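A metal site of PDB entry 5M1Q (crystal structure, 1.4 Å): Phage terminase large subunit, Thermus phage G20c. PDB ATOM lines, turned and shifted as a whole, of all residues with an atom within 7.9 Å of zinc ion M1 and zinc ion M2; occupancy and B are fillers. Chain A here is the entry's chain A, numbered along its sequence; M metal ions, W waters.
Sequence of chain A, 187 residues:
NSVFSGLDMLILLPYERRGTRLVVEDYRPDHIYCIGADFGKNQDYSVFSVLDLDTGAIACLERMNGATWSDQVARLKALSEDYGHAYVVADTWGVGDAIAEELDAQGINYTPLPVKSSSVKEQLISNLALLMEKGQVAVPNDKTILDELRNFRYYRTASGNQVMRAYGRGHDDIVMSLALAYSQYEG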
ATOM      1  N   ALA A  37      32.031 -23.371  30.877  1.00  0.00           N
ATOM      2  CA  ALA A  37      31.489 -22.256  30.075  1.00  0.00           C
ATOM      3  C   ALA A  37      31.181 -22.603  28.619  1.00  0.00           C
ATOM      4  O   ALA A  37      32.068 -23.029  27.869  1.00  0.00           O
ATOM      5  CB  ALA A  37      32.445 -21.077  30.121  1.00  0.00           C
ATOM      6  N   ASP A  38      29.912 -22.426  28.243  1.00  0.00           N
ATOM      7  CA  ASP A  38      29.396 -22.519  26.878  1.00  0.00           C
ATOM      8  C   ASP A  38      29.075 -21.067  26.434  1.00  0.00           C
ATOM      9  O   ASP A  38      28.728 -20.237  27.300  1.00  0.00           O
ATOM     10  CB  ASP A  38      28.136 -23.397  26.906  1.00  0.00           C
ATOM     11  CG  ASP A  38      27.647 -23.784  25.537  1.00  0.00           C
ATOM     12  OD1 ASP A  38      28.397 -24.421  24.778  1.00  0.00           O
ATOM     13  OD2 ASP A  38      26.482 -23.474  25.210  1.00  0.00           O
ATOM     14  N   PHE A  39      29.255 -20.750  25.143  1.00  0.00           N
ATOM     15  CA  PHE A  39      29.003 -19.386  24.611  1.00  0.00           C
ATOM     16  C   PHE A  39      27.984 -19.447  23.498  1.00  0.00           C
ATOM     17  O   PHE A  39      28.015 -20.387  22.684  1.00  0.00           O
ATOM     18  CB  PHE A  39      30.301 -18.787  24.064  1.00  0.00           C
ATOM     19  CG  PHE A  39      31.398 -18.716  25.089  1.00  0.00           C
ATOM     20  CD1 PHE A  39      31.416 -17.714  26.038  1.00  0.00           C
ATOM     21  CD2 PHE A  39      32.394 -19.669  25.113  1.00  0.00           C
ATOM     22  CE1 PHE A  39      32.420 -17.654  26.991  1.00  0.00           C
ATOM     23  CE2 PHE A  39      33.392 -19.630  26.075  1.00  0.00           C
ATOM     24  CZ  PHE A  39      33.406 -18.617  27.018  1.00  0.00           C
ATOM     25  N   GLY A  40      27.098 -18.450  23.450  1.00  0.00           N
ATOM     26  CA  GLY A  40      26.049 -18.379  22.427  1.00  0.00           C
ATOM     27  C   GLY A  40      26.386 -17.349  21.354  1.00  0.00           C
ATOM     28  O   GLY A  40      27.007 -16.322  21.662  1.00  0.00           O
ATOM     29  N   GLN A  43      20.699 -14.567  20.089  1.00  0.00           N
ATOM     30  CA  GLN A  43      19.545 -15.015  20.851  1.00  0.00           C
ATOM     31  C   GLN A  43      19.803 -16.404  21.478  1.00  0.00           C
ATOM     32  O   GLN A  43      19.013 -16.868  22.288  1.00  0.00           O
ATOM     33  CB  GLN A  43      18.269 -15.020  19.999  1.00  0.00           C
ATOM     34  CG  GLN A  43      17.770 -13.612  19.664  1.00  0.00           C
ATOM     35  CD  GLN A  43      17.115 -12.901  20.842  1.00  0.00           C
ATOM     36  OE1 GLN A  43      17.529 -11.795  21.212  1.00  0.00           O
ATOM     37  NE2 GLN A  43      16.103 -13.538  21.434  1.00  0.00           N
ATOM     38  N   ASP A  44      20.897 -17.064  21.068  1.00  0.00           N
ATOM     39  CA  ASP A  44      21.335 -18.310  21.738  1.00  0.00           C
ATOM     40  C   ASP A  44      21.976 -17.963  23.073  1.00  0.00           C
ATOM     41  O   ASP A  44      22.498 -16.847  23.268  1.00  0.00           O
ATOM     42  CB  ASP A  44      22.315 -19.125  20.869  1.00  0.00           C
ATOM     43  CG  ASP A  44      22.343 -20.609  21.260  1.00  0.00           C
ATOM     44  OD1 ASP A  44      21.461 -21.016  22.037  1.00  0.00           O
ATOM     45  OD2 ASP A  44      23.221 -21.362  20.775  1.00  0.00           O
ATOM     46  N   TYR A  45      21.948 -18.924  23.997  1.00  0.00           N
ATOM     47  CA  TYR A  45      22.361 -18.692  25.374  1.00  0.00           C
ATOM     48  C   TYR A  45      23.807 -19.050  25.642  1.00  0.00           C
ATOM     49  O   TYR A  45      24.327 -20.056  25.138  1.00  0.00           O
ATOM     50  CB  TYR A  45      21.495 -19.497  26.322  1.00  0.00           C
ATOM     51  CG  TYR A  45      20.079 -18.990  26.363  1.00  0.00           C
ATOM     52  CD1 TYR A  45      19.148 -19.397  25.404  1.00  0.00           C
ATOM     53  CD2 TYR A  45      19.675 -18.084  27.350  1.00  0.00           C
ATOM     54  CE1 TYR A  45      17.842 -18.905  25.435  1.00  0.00           C
ATOM     55  CE2 TYR A  45      18.382 -17.596  27.384  1.00  0.00           C
ATOM     56  CZ  TYR A  45      17.471 -18.013  26.424  1.00  0.00           C
ATOM     57  OH  TYR A  45      16.184 -17.532  26.455  1.00  0.00           O
ATOM     58  N   SER A  46      24.424 -18.222  26.480  1.00  0.00           N
ATOM     59  CA  SER A  46      25.670 -18.568  27.122  1.00  0.00           C
ATOM     60  C   SER A  46      25.364 -19.049  28.530  1.00  0.00           C
ATOM     61  O   SER A  46      24.482 -18.503  29.206  1.00  0.00           O
ATOM     62  CB  SER A  46      26.587 -17.368  27.169  1.00  0.00           C
ATOM     63  OG  SER A  46      26.786 -16.896  25.852  1.00  0.00           O
ATOM     64  N   VAL A  47      26.095 -20.072  28.980  1.00  0.00           N
ATOM     65  CA  VAL A  47      25.858 -20.622  30.323  1.00  0.00           C
ATOM     66  C   VAL A  47      27.174 -20.916  31.017  1.00  0.00           C
ATOM     67  O   VAL A  47      28.042 -21.605  30.470  1.00  0.00           O
ATOM     68  CB  VAL A  47      25.012 -21.906  30.263  1.00  0.00           C
ATOM     69  CG1 VAL A  47      24.766 -22.443  31.671  1.00  0.00           C
ATOM     70  CG2 VAL A  47      23.715 -21.699  29.478  1.00  0.00           C
ATOM     71  N   ARG A  63      23.133 -17.779  33.325  1.00  0.00           N
ATOM     72  CA  ARG A  63      22.646 -18.015  31.983  1.00  0.00           C
ATOM     73  C   ARG A  63      22.081 -16.719  31.420  1.00  0.00           C
ATOM     74  O   ARG A  63      21.339 -16.040  32.109  1.00  0.00           O
ATOM     75  CB  ARG A  63      21.566 -19.095  31.977  1.00  0.00           C
ATOM     76  CG  ARG A  63      20.919 -19.352  30.632  1.00  0.00           C
ATOM     77  CD  ARG A  63      20.084 -20.606  30.712  1.00  0.00           C
ATOM     78  NE  ARG A  63      19.429 -20.979  29.465  1.00  0.00           N
ATOM     79  CZ  ARG A  63      18.194 -20.656  29.089  1.00  0.00           C
ATOM     80  NH1 ARG A  63      17.411 -19.885  29.841  1.00  0.00           N
ATOM     81  NH2 ARG A  63      17.735 -21.109  27.918  1.00  0.00           N
ATOM     82  N   ASP A  91      34.487 -24.007  26.266  1.00  0.00           N
ATOM     83  CA  ASP A  91      34.324 -24.433  24.883  1.00  0.00           C
ATOM     84  C   ASP A  91      34.755 -23.261  23.969  1.00  0.00           C
ATOM     85  O   ASP A  91      33.973 -22.365  23.670  1.00  0.00           O
ATOM     86  CB  ASP A  91      32.883 -24.844  24.606  1.00  0.00           C
ATOM     87  CG  ASP A  91      32.675 -25.316  23.170  1.00  0.00           C
ATOM     88  OD1 ASP A  91      33.682 -25.467  22.437  1.00  0.00           O
ATOM     89  OD2 ASP A  91      31.516 -25.494  22.782  1.00  0.00           O
ATOM     90  N   GLU A 148      15.923 -28.918  29.952  1.00  0.00           N
ATOM     91  CA  GLU A 148      17.038 -29.191  29.041  1.00  0.00           C
ATOM     92  C   GLU A 148      17.610 -30.570  29.260  1.00  0.00           C
ATOM     93  O   GLU A 148      17.936 -31.245  28.308  1.00  0.00           O
ATOM     94  CB  GLU A 148      18.181 -28.154  29.173  1.00  0.00           C
ATOM     95  CG  GLU A 148      17.834 -26.787  28.601  1.00  0.00           C
ATOM     96  CD  GLU A 148      18.992 -25.988  28.028  1.00  0.00           C
ATOM     97  OE1 GLU A 148      20.146 -26.471  27.917  1.00  0.00           O
ATOM     98  OE2 GLU A 148      18.732 -24.832  27.674  1.00  0.00           O
ATOM     99  N   GLY A 170      15.306 -26.189  20.618  1.00  0.00           N
ATOM    100  CA  GLY A 170      15.661 -27.225  21.573  1.00  0.00           C
ATOM    101  C   GLY A 170      17.087 -27.070  22.081  1.00  0.00           C
ATOM    102  O   GLY A 170      17.993 -27.774  21.633  1.00  0.00           O
ATOM    103  N   HIS A 171      17.264 -26.150  23.022  1.00  0.00           N
ATOM    104  CA  HIS A 171      18.596 -25.758  23.503  1.00  0.00           C
ATOM    105  C   HIS A 171      19.253 -26.839  24.362  1.00  0.00           C
ATOM    106  O   HIS A 171      18.556 -27.569  25.085  1.00  0.00           O
ATOM    107  CB  HIS A 171      18.496 -24.507  24.366  1.00  0.00           C
ATOM    108  CG  HIS A 171      18.065 -23.284  23.625  1.00  0.00           C
ATOM    109  ND1 HIS A 171      18.842 -22.677  22.666  1.00  0.00           N
ATOM    110  CD2 HIS A 171      16.955 -22.507  23.750  1.00  0.00           C
ATOM    111  CE1 HIS A 171      18.221 -21.612  22.192  1.00  0.00           C
ATOM    112  NE2 HIS A 171      17.078 -21.486  22.831  1.00  0.00           N
ATOM    113  N   ASP A 172      20.573 -26.908  24.278  1.00  0.00           N
ATOM    114  CA  ASP A 172      21.394 -27.785  25.151  1.00  0.00           C
ATOM    115  C   ASP A 172      22.566 -27.034  25.799  1.00  0.00           C
ATOM    116  O   ASP A 172      23.491 -27.660  26.310  1.00  0.00           O
ATOM    117  CB  ASP A 172      21.904 -28.996  24.358  1.00  0.00           C
ATOM    118  CG  ASP A 172      23.019 -28.648  23.359  1.00  0.00           C
ATOM    119  OD1 ASP A 172      23.305 -27.454  23.093  1.00  0.00           O
ATOM    120  OD2 ASP A 172      23.630 -29.600  22.830  1.00  0.00           O
ATOM    121  N   ASP A 173      22.518 -25.702  25.839  1.00  0.00           N
ATOM    122  CA  ASP A 173      23.614 -24.915  26.388  1.00  0.00           C
ATOM    123  C   ASP A 173      23.860 -25.162  27.903  1.00  0.00           C
ATOM    124  O   ASP A 173      25.004 -25.149  28.359  1.00  0.00           O
ATOM    125  CB  ASP A 173      23.390 -23.424  26.189  1.00  0.00           C
ATOM    126  CG  ASP A 173      22.857 -23.113  24.833  1.00  0.00           C
ATOM    127  OD1 ASP A 173      23.653 -23.149  23.872  1.00  0.00           O
ATOM    128  OD2 ASP A 173      21.624 -22.933  24.746  1.00  0.00           O
ATOM    129  N   ILE A 174      22.784 -25.386  28.650  1.00  0.00           N
ATOM    130  CA  ILE A 174      22.907 -25.716  30.079  1.00  0.00           C
ATOM    131  C   ILE A 174      23.561 -27.077  30.239  1.00  0.00           C
ATOM    132  O   ILE A 174      24.479 -27.213  31.052  1.00  0.00           O
ATOM    133  CB  ILE A 174      21.550 -25.699  30.815  1.00  0.00           C
ATOM    134  CG1 ILE A 174      20.963 -24.281  30.769  1.00  0.00           C
ATOM    135  CG2 ILE A 174      21.684 -26.168  32.251  1.00  0.00           C
ATOM    136  CD1 ILE A 174      19.495 -24.237  31.102  1.00  0.00           C
ATOM    137  N   MET A 176      25.578 -28.638  28.186  1.00  0.00           N
ATOM    138  CA  MET A 176      26.988 -28.567  27.839  1.00  0.00           C
ATOM    139  C   MET A 176      27.828 -27.869  28.901  1.00  0.00           C
ATOM    140  O   MET A 176      28.922 -28.299  29.220  1.00  0.00           O
ATOM    141  CB  MET A 176      27.175 -27.941  26.464  1.00  0.00           C
ATOM    142  CG  MET A 176      26.596 -28.796  25.348  1.00  0.00           C
ATOM    143  SD  MET A 176      27.204 -30.508  25.341  1.00  0.00           S
ATOM    144  CE  MET A 176      28.969 -30.273  25.322  1.00  0.00           C
ATOM    145  N   SER A 177      27.302 -26.781  29.462  1.00  0.00           N
ATOM    146  CA  SER A 177      28.006 -26.098  30.520  1.00  0.00           C
ATOM    147  C   SER A 177      28.209 -26.989  31.761  1.00  0.00           C
ATOM    148  O   SER A 177      29.288 -27.066  32.336  1.00  0.00           O
ATOM    149  CB  SER A 177      27.226 -24.851  30.900  1.00  0.00           C
ATOM    150  OG  SER A 177      27.790 -24.218  32.015  1.00  0.00           O
HETATM  151 ZN    ZN M   1      21.017 -22.853  22.733  1.00  0.00          ZN
HETATM  152 ZN    ZN M   2      25.521 -23.582  23.276  1.00  0.00          ZN
HETATM  153  O   HOH W   1      25.385 -25.635  23.350  1.00  0.00           O
HETATM  154  O   HOH W   2      24.471 -23.631  21.264  1.00  0.00           O
HETATM  155  O   HOH W   3      21.494 -24.766  21.745  1.00  0.00           O
HETATM  156  O   HOH W   4      25.827 -21.664  23.634  1.00  0.00           O
HETATM  157  O   HOH W   5      27.268 -23.532  22.392  1.00  0.00           O
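OE1 of Glu 148 lies within hydrogen-bond range of N of Asp 173. N of Asp 38 lies within hydrogen-bond range of O of Val 47, 3.0 Å away.
Of the 19 residues printed, 3 come within 4 Å of zinc ion M1.
Of the 19 residues printed, 2 come within 4 Å of zinc ion M2. The nearest printed residue that does not touch zinc ion M2 is Asp 44 (4.1 Å).
Zinc ion M1 is bound by the side-chain carboxylate (OD1) of Asp 44, 2.0 Å away. Zinc ion M1 is bound by OD2 of Asp 173. Zinc ion M1 is bound by ND1 of His 171 (2.2 Å). Water W3 binds zinc ion M1, at 2.2 Å.
Zinc ion M2 is bound by water W5 (2.0 Å), water W4 (2.0 Å), OD1 of Asp 173 (2.0 Å), water W1 (2.1 Å), OD2 of Asp 38 (2.2 Å) and water W2 (2.3 Å). Zinc ion M2 has six donor atoms within binding distance.
Water W5 lies within hydrogen-bond range of the side-chain carboxylate (OD1) of Asp 38 and the backbone carbonyl oxygen (O) of Phe 39. Water W4 lies within hydrogen-bond range of O of Tyr 45 (2.7 Å), O of Phe 39 (2.7 Å) and N of Gly 40 (3.5 Å).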
